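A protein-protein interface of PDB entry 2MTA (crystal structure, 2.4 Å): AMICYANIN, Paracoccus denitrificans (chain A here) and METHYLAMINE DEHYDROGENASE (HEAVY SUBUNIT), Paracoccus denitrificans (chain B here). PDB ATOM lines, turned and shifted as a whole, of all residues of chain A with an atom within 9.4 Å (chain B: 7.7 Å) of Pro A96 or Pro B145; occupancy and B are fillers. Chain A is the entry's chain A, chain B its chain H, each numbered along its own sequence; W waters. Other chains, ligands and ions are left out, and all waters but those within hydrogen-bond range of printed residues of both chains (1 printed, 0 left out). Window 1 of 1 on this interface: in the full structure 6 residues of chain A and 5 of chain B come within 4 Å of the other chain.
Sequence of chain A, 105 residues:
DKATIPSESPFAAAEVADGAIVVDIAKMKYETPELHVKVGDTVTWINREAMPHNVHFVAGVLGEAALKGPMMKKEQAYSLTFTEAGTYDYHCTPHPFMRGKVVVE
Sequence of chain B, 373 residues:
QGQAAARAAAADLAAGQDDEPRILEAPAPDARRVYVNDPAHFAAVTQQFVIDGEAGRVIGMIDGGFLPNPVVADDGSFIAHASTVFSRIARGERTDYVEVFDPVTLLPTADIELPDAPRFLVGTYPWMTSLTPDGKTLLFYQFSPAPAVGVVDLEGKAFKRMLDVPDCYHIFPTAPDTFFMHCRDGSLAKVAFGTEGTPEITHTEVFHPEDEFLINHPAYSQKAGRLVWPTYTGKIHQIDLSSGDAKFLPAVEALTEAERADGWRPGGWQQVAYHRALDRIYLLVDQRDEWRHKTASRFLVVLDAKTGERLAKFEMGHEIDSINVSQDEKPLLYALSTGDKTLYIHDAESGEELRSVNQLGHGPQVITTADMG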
ATOM      1  N   MET A  28     -33.646   1.174  28.578  1.00  0.00           N
ATOM      2  CA  MET A  28     -32.228   0.845  28.748  1.00  0.00           C
ATOM      3  C   MET A  28     -31.905  -0.570  28.365  1.00  0.00           C
ATOM      4  O   MET A  28     -30.980  -1.168  28.928  1.00  0.00           O
ATOM      5  CB  MET A  28     -31.803   1.102  30.184  1.00  0.00           C
ATOM      6  CG  MET A  28     -31.917   2.560  30.660  1.00  0.00           C
ATOM      7  SD  MET A  28     -30.760   3.722  29.877  1.00  0.00           S
ATOM      8  CE  MET A  28     -29.275   2.843  30.236  1.00  0.00           C
ATOM      9  N   TYR A  30     -31.797  -3.749  25.061  1.00  0.00           N
ATOM     10  CA  TYR A  30     -31.996  -4.394  23.774  1.00  0.00           C
ATOM     11  C   TYR A  30     -33.071  -5.443  23.959  1.00  0.00           C
ATOM     12  O   TYR A  30     -32.812  -6.564  24.429  1.00  0.00           O
ATOM     13  CB  TYR A  30     -30.773  -5.113  23.295  1.00  0.00           C
ATOM     14  CG  TYR A  30     -29.632  -4.167  22.999  1.00  0.00           C
ATOM     15  CD1 TYR A  30     -29.700  -3.236  21.984  1.00  0.00           C
ATOM     16  CD2 TYR A  30     -28.502  -4.237  23.774  1.00  0.00           C
ATOM     17  CE1 TYR A  30     -28.623  -2.377  21.759  1.00  0.00           C
ATOM     18  CE2 TYR A  30     -27.433  -3.398  23.547  1.00  0.00           C
ATOM     19  CZ  TYR A  30     -27.493  -2.474  22.553  1.00  0.00           C
ATOM     20  OH  TYR A  30     -26.414  -1.650  22.368  1.00  0.00           O
ATOM     21  N   HIS A  53     -28.654   5.862  22.213  1.00  0.00           N
ATOM     22  CA  HIS A  53     -28.010   4.556  22.381  1.00  0.00           C
ATOM     23  C   HIS A  53     -27.392   4.151  21.063  1.00  0.00           C
ATOM     24  O   HIS A  53     -27.910   4.572  20.043  1.00  0.00           O
ATOM     25  CB  HIS A  53     -29.006   3.385  22.738  1.00  0.00           C
ATOM     26  CG  HIS A  53     -29.786   3.462  24.053  1.00  0.00           C
ATOM     27  ND1 HIS A  53     -29.155   3.440  25.202  1.00  0.00           N
ATOM     28  CD2 HIS A  53     -31.131   3.705  24.167  1.00  0.00           C
ATOM     29  CE1 HIS A  53     -30.083   3.687  26.094  1.00  0.00           C
ATOM     30  NE2 HIS A  53     -31.224   3.846  25.473  1.00  0.00           N
ATOM     31  N   ASN A  54     -26.434   3.227  21.027  1.00  0.00           N
ATOM     32  CA  ASN A  54     -25.879   2.766  19.761  1.00  0.00           C
ATOM     33  C   ASN A  54     -25.652   1.271  19.835  1.00  0.00           C
ATOM     34  O   ASN A  54     -26.135   0.669  20.788  1.00  0.00           O
ATOM     35  CB  ASN A  54     -24.555   3.470  19.496  1.00  0.00           C
ATOM     36  CG  ASN A  54     -23.369   3.089  20.351  1.00  0.00           C
ATOM     37  OD1 ASN A  54     -23.446   2.760  21.551  1.00  0.00           O
ATOM     38  ND2 ASN A  54     -22.201   3.174  19.709  1.00  0.00           N
ATOM     39  N   HIS A  56     -22.258  -1.536  19.480  1.00  0.00           N
ATOM     40  CA  HIS A  56     -20.840  -1.445  19.339  1.00  0.00           C
ATOM     41  C   HIS A  56     -20.314  -2.865  19.457  1.00  0.00           C
ATOM     42  O   HIS A  56     -20.475  -3.526  20.482  1.00  0.00           O
ATOM     43  CB  HIS A  56     -20.422  -0.463  20.438  1.00  0.00           C
ATOM     44  CG  HIS A  56     -18.959  -0.297  20.849  1.00  0.00           C
ATOM     45  ND1 HIS A  56     -18.525   0.554  21.795  1.00  0.00           N
ATOM     46  CD2 HIS A  56     -17.869  -1.051  20.421  1.00  0.00           C
ATOM     47  CE1 HIS A  56     -17.242   0.322  21.966  1.00  0.00           C
ATOM     48  NE2 HIS A  56     -16.849  -0.640  21.144  1.00  0.00           N
ATOM     49  N   PHE A  57     -19.723  -3.368  18.394  1.00  0.00           N
ATOM     50  CA  PHE A  57     -19.110  -4.695  18.377  1.00  0.00           C
ATOM     51  C   PHE A  57     -17.617  -4.482  18.597  1.00  0.00           C
ATOM     52  O   PHE A  57     -17.055  -3.583  17.972  1.00  0.00           O
ATOM     53  CB  PHE A  57     -19.333  -5.369  17.018  1.00  0.00           C
ATOM     54  CG  PHE A  57     -20.818  -5.567  16.719  1.00  0.00           C
ATOM     55  CD1 PHE A  57     -21.549  -4.484  16.313  1.00  0.00           C
ATOM     56  CD2 PHE A  57     -21.427  -6.824  16.878  1.00  0.00           C
ATOM     57  CE1 PHE A  57     -22.908  -4.636  16.070  1.00  0.00           C
ATOM     58  CE2 PHE A  57     -22.770  -6.954  16.622  1.00  0.00           C
ATOM     59  CZ  PHE A  57     -23.514  -5.862  16.224  1.00  0.00           C
ATOM     60  N   VAL A  58     -16.869  -5.199  19.409  1.00  0.00           N
ATOM     61  CA  VAL A  58     -15.488  -4.807  19.550  1.00  0.00           C
ATOM     62  C   VAL A  58     -14.689  -5.542  18.499  1.00  0.00           C
ATOM     63  O   VAL A  58     -15.204  -6.279  17.639  1.00  0.00           O
ATOM     64  CB  VAL A  58     -14.943  -5.102  20.964  1.00  0.00           C
ATOM     65  CG1 VAL A  58     -15.847  -4.497  22.080  1.00  0.00           C
ATOM     66  CG2 VAL A  58     -14.779  -6.580  21.072  1.00  0.00           C
ATOM     67  N   ALA A  59     -13.429  -5.149  18.504  1.00  0.00           N
ATOM     68  CA  ALA A  59     -12.433  -5.675  17.576  1.00  0.00           C
ATOM     69  C   ALA A  59     -12.337  -7.198  17.559  1.00  0.00           C
ATOM     70  O   ALA A  59     -12.271  -7.909  18.563  1.00  0.00           O
ATOM     71  CB  ALA A  59     -11.051  -5.111  17.924  1.00  0.00           C
ATOM     72  N   ALA A  66     -13.182  -2.808  15.524  1.00  0.00           N
ATOM     73  CA  ALA A  66     -14.381  -2.688  16.318  1.00  0.00           C
ATOM     74  C   ALA A  66     -15.310  -1.867  15.476  1.00  0.00           C
ATOM     75  O   ALA A  66     -14.776  -1.013  14.761  1.00  0.00           O
ATOM     76  CB  ALA A  66     -14.115  -1.907  17.592  1.00  0.00           C
ATOM     77  N   LYS A  68     -18.006   0.894  16.212  1.00  0.00           N
ATOM     78  CA  LYS A  68     -18.826   1.621  17.162  1.00  0.00           C
ATOM     79  C   LYS A  68     -19.867   2.155  16.223  1.00  0.00           C
ATOM     80  O   LYS A  68     -19.452   2.806  15.268  1.00  0.00           O
ATOM     81  CB  LYS A  68     -18.254   2.869  17.779  1.00  0.00           C
ATOM     82  CG  LYS A  68     -17.212   2.758  18.863  1.00  0.00           C
ATOM     83  CD  LYS A  68     -15.772   2.525  18.364  1.00  0.00           C
ATOM     84  CE  LYS A  68     -14.802   2.837  19.517  1.00  0.00           C
ATOM     85  NZ  LYS A  68     -13.504   2.199  19.371  1.00  0.00           N
ATOM     86  N   ASP A  89     -21.407 -10.683  19.522  1.00  0.00           N
ATOM     87  CA  ASP A  89     -21.820  -9.974  20.718  1.00  0.00           C
ATOM     88  C   ASP A  89     -21.555  -8.492  20.570  1.00  0.00           C
ATOM     89  O   ASP A  89     -20.524  -8.116  20.005  1.00  0.00           O
ATOM     90  CB  ASP A  89     -21.046 -10.440  21.961  1.00  0.00           C
ATOM     91  CG  ASP A  89     -21.140 -11.932  22.269  1.00  0.00           C
ATOM     92  OD1 ASP A  89     -20.339 -12.740  21.781  1.00  0.00           O
ATOM     93  OD2 ASP A  89     -22.041 -12.288  23.022  1.00  0.00           O
ATOM     94  N   TYR A  90     -22.465  -7.690  21.122  1.00  0.00           N
ATOM     95  CA  TYR A  90     -22.397  -6.244  21.131  1.00  0.00           C
ATOM     96  C   TYR A  90     -22.874  -5.633  22.426  1.00  0.00           C
ATOM     97  O   TYR A  90     -23.614  -6.266  23.176  1.00  0.00           O
ATOM     98  CB  TYR A  90     -23.244  -5.655  20.023  1.00  0.00           C
ATOM     99  CG  TYR A  90     -24.737  -5.932  19.999  1.00  0.00           C
ATOM    100  CD1 TYR A  90     -25.229  -7.105  19.455  1.00  0.00           C
ATOM    101  CD2 TYR A  90     -25.595  -5.022  20.549  1.00  0.00           C
ATOM    102  CE1 TYR A  90     -26.593  -7.392  19.464  1.00  0.00           C
ATOM    103  CE2 TYR A  90     -26.951  -5.298  20.585  1.00  0.00           C
ATOM    104  CZ  TYR A  90     -27.442  -6.479  20.041  1.00  0.00           C
ATOM    105  OH  TYR A  90     -28.795  -6.743  20.100  1.00  0.00           O
ATOM    106  N   HIS A  91     -22.481  -4.395  22.698  1.00  0.00           N
ATOM    107  CA  HIS A  91     -22.967  -3.632  23.839  1.00  0.00           C
ATOM    108  C   HIS A  91     -23.213  -2.205  23.392  1.00  0.00           C
ATOM    109  O   HIS A  91     -23.073  -1.883  22.219  1.00  0.00           O
ATOM    110  CB  HIS A  91     -21.959  -3.618  24.929  1.00  0.00           C
ATOM    111  CG  HIS A  91     -20.702  -2.817  24.582  1.00  0.00           C
ATOM    112  ND1 HIS A  91     -19.758  -3.204  23.740  1.00  0.00           N
ATOM    113  CD2 HIS A  91     -20.407  -1.568  25.106  1.00  0.00           C
ATOM    114  CE1 HIS A  91     -18.894  -2.232  23.730  1.00  0.00           C
ATOM    115  NE2 HIS A  91     -19.279  -1.258  24.543  1.00  0.00           N
ATOM    116  N   CYS A  92     -23.587  -1.283  24.246  1.00  0.00           N
ATOM    117  CA  CYS A  92     -23.856   0.062  23.910  1.00  0.00           C
ATOM    118  C   CYS A  92     -22.690   0.830  24.453  1.00  0.00           C
ATOM    119  O   CYS A  92     -22.496   0.857  25.647  1.00  0.00           O
ATOM    120  CB  CYS A  92     -25.038   0.488  24.593  1.00  0.00           C
ATOM    121  SG  CYS A  92     -25.464   2.186  24.098  1.00  0.00           S
ATOM    122  N   THR A  93     -21.977   1.576  23.656  1.00  0.00           N
ATOM    123  CA  THR A  93     -20.817   2.368  24.051  1.00  0.00           C
ATOM    124  C   THR A  93     -20.985   3.238  25.294  1.00  0.00           C
ATOM    125  O   THR A  93     -20.153   3.051  26.190  1.00  0.00           O
ATOM    126  CB  THR A  93     -20.433   3.218  22.804  1.00  0.00           C
ATOM    127  OG1 THR A  93     -20.435   2.389  21.607  1.00  0.00           O
ATOM    128  CG2 THR A  93     -19.105   3.823  23.004  1.00  0.00           C
ATOM    129  N   PRO A  94     -21.954   4.156  25.513  1.00  0.00           N
ATOM    130  CA  PRO A  94     -21.990   4.899  26.763  1.00  0.00           C
ATOM    131  C   PRO A  94     -22.490   4.136  27.975  1.00  0.00           C
ATOM    132  O   PRO A  94     -22.376   4.516  29.134  1.00  0.00           O
ATOM    133  CB  PRO A  94     -22.851   6.124  26.458  1.00  0.00           C
ATOM    134  CG  PRO A  94     -23.769   5.632  25.378  1.00  0.00           C
ATOM    135  CD  PRO A  94     -22.869   4.717  24.536  1.00  0.00           C
ATOM    136  N   HIS A  95     -23.108   2.997  27.681  1.00  0.00           N
ATOM    137  CA  HIS A  95     -23.878   2.202  28.675  1.00  0.00           C
ATOM    138  C   HIS A  95     -23.508   0.708  28.575  1.00  0.00           C
ATOM    139  O   HIS A  95     -24.351  -0.049  28.081  1.00  0.00           O
ATOM    140  CB  HIS A  95     -25.390   2.427  28.394  1.00  0.00           C
ATOM    141  CG  HIS A  95     -25.819   3.895  28.261  1.00  0.00           C
ATOM    142  ND1 HIS A  95     -26.599   4.249  27.285  1.00  0.00           N
ATOM    143  CD2 HIS A  95     -25.604   4.920  29.125  1.00  0.00           C
ATOM    144  CE1 HIS A  95     -26.931   5.486  27.474  1.00  0.00           C
ATOM    145  NE2 HIS A  95     -26.330   5.868  28.570  1.00  0.00           N
ATOM    146  N   PRO A  96     -22.311   0.198  28.954  1.00  0.00           N
ATOM    147  CA  PRO A  96     -21.859  -1.141  28.652  1.00  0.00           C
ATOM    148  C   PRO A  96     -22.574  -2.253  29.416  1.00  0.00           C
ATOM    149  O   PRO A  96     -22.333  -3.422  29.182  1.00  0.00           O
ATOM    150  CB  PRO A  96     -20.366  -1.074  28.884  1.00  0.00           C
ATOM    151  CG  PRO A  96     -20.173  -0.071  29.944  1.00  0.00           C
ATOM    152  CD  PRO A  96     -21.307   0.914  29.748  1.00  0.00           C
ATOM    153  N   PHE A  97     -23.492  -1.952  30.332  1.00  0.00           N
ATOM    154  CA  PHE A  97     -24.382  -2.950  30.917  1.00  0.00           C
ATOM    155  C   PHE A  97     -25.525  -3.278  29.942  1.00  0.00           C
ATOM    156  O   PHE A  97     -26.382  -4.113  30.244  1.00  0.00           O
ATOM    157  CB  PHE A  97     -25.000  -2.435  32.256  1.00  0.00           C
ATOM    158  CG  PHE A  97     -25.595  -1.053  32.132  1.00  0.00           C
ATOM    159  CD1 PHE A  97     -24.775   0.032  32.344  1.00  0.00           C
ATOM    160  CD2 PHE A  97     -26.926  -0.869  31.742  1.00  0.00           C
ATOM    161  CE1 PHE A  97     -25.302   1.306  32.157  1.00  0.00           C
ATOM    162  CE2 PHE A  97     -27.433   0.409  31.559  1.00  0.00           C
ATOM    163  CZ  PHE A  97     -26.615   1.509  31.764  1.00  0.00           C
ATOM    164  N   MET A  98     -25.649  -2.602  28.789  1.00  0.00           N
ATOM    165  CA  MET A  98     -26.699  -2.919  27.814  1.00  0.00           C
ATOM    166  C   MET A  98     -26.047  -3.855  26.800  1.00  0.00           C
ATOM    167  O   MET A  98     -25.122  -3.432  26.113  1.00  0.00           O
ATOM    168  CB  MET A  98     -27.160  -1.669  27.108  1.00  0.00           C
ATOM    169  CG  MET A  98     -28.037  -0.808  27.952  1.00  0.00           C
ATOM    170  SD  MET A  98     -28.708   0.484  26.867  1.00  0.00           S
ATOM    171  CE  MET A  98     -29.219  -0.368  25.407  1.00  0.00           C
ATOM    172  N   ARG A  99     -26.436  -5.121  26.683  1.00  0.00           N
ATOM    173  CA  ARG A  99     -25.803  -6.099  25.800  1.00  0.00           C
ATOM    174  C   ARG A  99     -26.802  -6.888  24.988  1.00  0.00           C
ATOM    175  O   ARG A  99     -27.993  -6.906  25.304  1.00  0.00           O
ATOM    176  CB  ARG A  99     -24.994  -7.070  26.585  1.00  0.00           C
ATOM    177  CG  ARG A  99     -23.829  -6.368  27.254  1.00  0.00           C
ATOM    178  CD  ARG A  99     -22.931  -7.281  28.060  1.00  0.00           C
ATOM    179  NE  ARG A  99     -23.369  -7.268  29.429  1.00  0.00           N
ATOM    180  CZ  ARG A  99     -22.689  -6.680  30.416  1.00  0.00           C
ATOM    181  NH1 ARG A  99     -21.535  -6.009  30.299  1.00  0.00           N
ATOM    182  NH2 ARG A  99     -23.292  -6.685  31.575  1.00  0.00           N
ATOM    183  N   GLY A 100     -26.339  -7.564  23.953  1.00  0.00           N
ATOM    184  CA  GLY A 100     -27.161  -8.351  23.079  1.00  0.00           C
ATOM    185  C   GLY A 100     -26.245  -9.236  22.280  1.00  0.00           C
ATOM    186  O   GLY A 100     -25.029  -9.219  22.425  1.00  0.00           O
ATOM    187  N   ASP B 116      -2.802  -1.719  25.976  1.00  0.00           N
ATOM    188  CA  ASP B 116      -3.984  -1.313  25.254  1.00  0.00           C
ATOM    189  C   ASP B 116      -4.749  -0.253  25.977  1.00  0.00           C
ATOM    190  O   ASP B 116      -5.957  -0.147  25.836  1.00  0.00           O
ATOM    191  CB  ASP B 116      -4.907  -2.525  25.006  1.00  0.00           C
ATOM    192  CG  ASP B 116      -4.281  -3.712  24.261  1.00  0.00           C
ATOM    193  OD1 ASP B 116      -3.359  -3.520  23.446  1.00  0.00           O
ATOM    194  OD2 ASP B 116      -4.727  -4.840  24.517  1.00  0.00           O
ATOM    195  N   ALA B 117      -4.036   0.582  26.715  1.00  0.00           N
ATOM    196  CA  ALA B 117      -4.684   1.692  27.369  1.00  0.00           C
ATOM    197  C   ALA B 117      -6.043   1.456  28.040  1.00  0.00           C
ATOM    198  O   ALA B 117      -7.099   1.906  27.583  1.00  0.00           O
ATOM    199  CB  ALA B 117      -4.778   2.801  26.322  1.00  0.00           C
ATOM    200  N   PRO B 118      -6.065   0.780  29.179  1.00  0.00           N
ATOM    201  CA  PRO B 118      -7.309   0.325  29.671  1.00  0.00           C
ATOM    202  C   PRO B 118      -7.762   1.145  30.823  1.00  0.00           C
ATOM    203  O   PRO B 118      -8.857   0.868  31.272  1.00  0.00           O
ATOM    204  CB  PRO B 118      -7.007  -1.106  29.937  1.00  0.00           C
ATOM    205  CG  PRO B 118      -5.577  -1.102  30.430  1.00  0.00           C
ATOM    206  CD  PRO B 118      -4.952   0.117  29.832  1.00  0.00           C
ATOM    207  N   TYR B 141      -9.781  -0.268  37.772  1.00  0.00           N
ATOM    208  CA  TYR B 141     -11.027  -0.458  37.101  1.00  0.00           C
ATOM    209  C   TYR B 141     -11.006  -0.125  35.626  1.00  0.00           C
ATOM    210  O   TYR B 141     -10.394   0.852  35.276  1.00  0.00           O
ATOM    211  CB  TYR B 141     -12.094   0.396  37.773  1.00  0.00           C
ATOM    212  CG  TYR B 141     -13.493   0.095  37.232  1.00  0.00           C
ATOM    213  CD1 TYR B 141     -14.066  -1.158  37.485  1.00  0.00           C
ATOM    214  CD2 TYR B 141     -14.221   1.013  36.502  1.00  0.00           C
ATOM    215  CE1 TYR B 141     -15.341  -1.479  37.019  1.00  0.00           C
ATOM    216  CE2 TYR B 141     -15.507   0.690  36.037  1.00  0.00           C
ATOM    217  CZ  TYR B 141     -16.061  -0.557  36.286  1.00  0.00           C
ATOM    218  OH  TYR B 141     -17.317  -0.920  35.827  1.00  0.00           O
ATOM    219  N   GLN B 142     -11.703  -0.844  34.750  1.00  0.00           N
ATOM    220  CA  GLN B 142     -11.861  -0.548  33.325  1.00  0.00           C
ATOM    221  C   GLN B 142     -13.337  -0.554  33.134  1.00  0.00           C
ATOM    222  O   GLN B 142     -13.988  -1.510  33.516  1.00  0.00           O
ATOM    223  CB  GLN B 142     -11.307  -1.621  32.408  1.00  0.00           C
ATOM    224  CG  GLN B 142     -11.639  -1.399  30.933  1.00  0.00           C
ATOM    225  CD  GLN B 142     -11.207  -2.566  30.065  1.00  0.00           C
ATOM    226  OE1 GLN B 142     -10.117  -2.656  29.506  1.00  0.00           O
ATOM    227  NE2 GLN B 142     -12.104  -3.540  29.923  1.00  0.00           N
ATOM    228  N   PHE B 143     -13.856   0.448  32.477  1.00  0.00           N
ATOM    229  CA  PHE B 143     -15.261   0.643  32.299  1.00  0.00           C
ATOM    230  C   PHE B 143     -15.587   0.257  30.885  1.00  0.00           C
ATOM    231  O   PHE B 143     -16.655  -0.270  30.653  1.00  0.00           O
ATOM    232  CB  PHE B 143     -15.523   2.088  32.562  1.00  0.00           C
ATOM    233  CG  PHE B 143     -16.886   2.608  32.238  1.00  0.00           C
ATOM    234  CD1 PHE B 143     -17.911   2.531  33.165  1.00  0.00           C
ATOM    235  CD2 PHE B 143     -17.147   3.136  30.990  1.00  0.00           C
ATOM    236  CE1 PHE B 143     -19.188   2.969  32.815  1.00  0.00           C
ATOM    237  CE2 PHE B 143     -18.428   3.576  30.657  1.00  0.00           C
ATOM    238  CZ  PHE B 143     -19.441   3.488  31.564  1.00  0.00           C
ATOM    239  N   SER B 144     -14.775   0.486  29.874  1.00  0.00           N
ATOM    240  CA  SER B 144     -15.232   0.283  28.509  1.00  0.00           C
ATOM    241  C   SER B 144     -14.082  -0.493  27.959  1.00  0.00           C
ATOM    242  O   SER B 144     -12.947  -0.263  28.365  1.00  0.00           O
ATOM    243  CB  SER B 144     -15.418   1.655  27.818  1.00  0.00           C
ATOM    244  OG  SER B 144     -15.642   1.722  26.402  1.00  0.00           O
ATOM    245  N   PRO B 145     -14.331  -1.478  27.103  1.00  0.00           N
ATOM    246  CA  PRO B 145     -15.660  -1.746  26.531  1.00  0.00           C
ATOM    247  C   PRO B 145     -16.616  -2.606  27.348  1.00  0.00           C
ATOM    248  O   PRO B 145     -17.743  -2.902  26.934  1.00  0.00           O
ATOM    249  CB  PRO B 145     -15.316  -2.339  25.225  1.00  0.00           C
ATOM    250  CG  PRO B 145     -14.075  -3.184  25.511  1.00  0.00           C
ATOM    251  CD  PRO B 145     -13.287  -2.305  26.495  1.00  0.00           C
ATOM    252  N   ALA B 146     -16.200  -2.967  28.559  1.00  0.00           N
ATOM    253  CA  ALA B 146     -16.929  -3.951  29.351  1.00  0.00           C
ATOM    254  C   ALA B 146     -16.276  -3.849  30.698  1.00  0.00           C
ATOM    255  O   ALA B 146     -15.052  -3.602  30.678  1.00  0.00           O
ATOM    256  CB  ALA B 146     -16.689  -5.353  28.805  1.00  0.00           C
ATOM    257  N   PRO B 147     -16.980  -4.007  31.824  1.00  0.00           N
ATOM    258  CA  PRO B 147     -16.416  -3.889  33.159  1.00  0.00           C
ATOM    259  C   PRO B 147     -15.315  -4.880  33.386  1.00  0.00           C
ATOM    260  O   PRO B 147     -15.469  -6.027  32.972  1.00  0.00           O
ATOM    261  CB  PRO B 147     -17.623  -4.048  34.089  1.00  0.00           C
ATOM    262  CG  PRO B 147     -18.563  -4.831  33.255  1.00  0.00           C
ATOM    263  CD  PRO B 147     -18.426  -4.186  31.885  1.00  0.00           C
ATOM    264  N   ALA B 148     -14.162  -4.486  33.929  1.00  0.00           N
ATOM    265  CA  ALA B 148     -13.063  -5.425  34.133  1.00  0.00           C
ATOM    266  C   ALA B 148     -12.108  -4.854  35.111  1.00  0.00           C
ATOM    267  O   ALA B 148     -12.161  -3.622  35.291  1.00  0.00           O
ATOM    268  CB  ALA B 148     -12.276  -5.656  32.902  1.00  0.00           C
ATOM    269  N   ASP B 167     -21.555  -5.743  36.068  1.00  0.00           N
ATOM    270  CA  ASP B 167     -21.770  -4.310  36.087  1.00  0.00           C
ATOM    271  C   ASP B 167     -21.762  -3.747  37.479  1.00  0.00           C
ATOM    272  O   ASP B 167     -22.779  -3.394  38.073  1.00  0.00           O
ATOM    273  CB  ASP B 167     -23.050  -4.029  35.410  1.00  0.00           C
ATOM    274  CG  ASP B 167     -23.017  -4.801  34.114  1.00  0.00           C
ATOM    275  OD1 ASP B 167     -22.397  -4.380  33.144  1.00  0.00           O
ATOM    276  OD2 ASP B 167     -23.573  -5.886  34.138  1.00  0.00           O
ATOM    277  N   TYR B 169     -18.837  -1.403  40.231  1.00  0.00           N
ATOM    278  CA  TYR B 169     -17.902  -0.279  40.263  1.00  0.00           C
ATOM    279  C   TYR B 169     -17.187  -0.175  41.614  1.00  0.00           C
ATOM    280  O   TYR B 169     -17.871  -0.449  42.586  1.00  0.00           O
ATOM    281  CB  TYR B 169     -18.695   1.030  39.990  1.00  0.00           C
ATOM    282  CG  TYR B 169     -19.557   0.920  38.729  1.00  0.00           C
ATOM    283  CD1 TYR B 169     -20.822   0.383  38.805  1.00  0.00           C
ATOM    284  CD2 TYR B 169     -19.037   1.279  37.502  1.00  0.00           C
ATOM    285  CE1 TYR B 169     -21.524   0.228  37.640  1.00  0.00           C
ATOM    286  CE2 TYR B 169     -19.746   1.101  36.333  1.00  0.00           C
ATOM    287  CZ  TYR B 169     -20.987   0.581  36.420  1.00  0.00           C
ATOM    288  OH  TYR B 169     -21.707   0.382  35.265  1.00  0.00           O
HETATM  289  O   HOH W   1     -20.259  -4.599  27.546  1.00  0.00           O
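The backbone carbonyl oxygen of Pro B145 lies within hydrogen-bond range of a ring nitrogen (NE2) of His A91.
The side-chain carboxylate of Asp B167 is in salt-bridge range of the guanidinium group of Arg A99 (2.7 Å).
The guanidinium group of Arg A99 is in hydrogen-bond range of the backbone carbonyl oxygen of Pro A96, 2.9 Å away.
The backbone carbonyl oxygen (O) of His A91 lies within hydrogen-bond range of the side-chain hydroxyl (OH) of Tyr A30, at 3.4 Å.
N of His A56 sits at hydrogen-bond distance from O of His A91, 2.9 Å away.
Among the printed residues, pairs that only touch across the chains: Val A58 with Pro B145 (3.9 Å), Pro A94 with Phe B143 (3.9 Å), Pro A96 with Phe B143 (3.6 Å), Pro A96 with Pro B145 (3.7 Å), Phe A97 with Asp B167 (3.3 Å) and Arg A99 with Pro B147 (3.9 Å).
Of the printed residues of chain B, Val A58 touches Pro B145 (3.9 Å).
Pro A96 touches just these residues of chain B: Phe B143 (3.6 Å) and Pro B145 (3.7 Å).
Printed residues of chain B within 4 Å of Phe A97: Asp B167 (3.3 Å).
Printed residues of chain A within 4 Å of Phe B143: Pro A94 and Pro A96.
Of chain A, only Val A58, His A91 and Pro A96 come within 4 Å of Pro B145.
No residue of chain A comes within 4 Å of Ala B146.
Printed residues of chain A within 4 Å of Pro B147: Arg A99.
Of the printed residues of chain A, Asp B167 touches Phe A97 (3.3 Å) and Arg A99 (2.7 Å).
The nearest residue of chain A that does not touch Pro B145 is His A56 (4.6 Å).
The nearest printed residue of chain B that does not touch Phe A97 is Tyr B169 (4.3 Å).
Of the 22 printed residues of chain A, 6 touch a printed residue of chain B.
Of the 13 printed residues of chain B, 4 touch a printed residue of chain A.
Printed residues of chain B that touch a printed residue of chain A: Phe B143, Pro B145, Pro B147 and Asp B167.
Among the printed residues, 8 pairs touch across the chains.
Among the printed residues, Asp or Glu carboxylates within 4 Å of a Lys or Arg side-chain nitrogen of the other chain: Arg A99 with Asp B167 (2.7 Å).
Water W1 lies within hydrogen-bond range of O of Pro A96, O of Pro B145 and NH1 of Arg A99.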
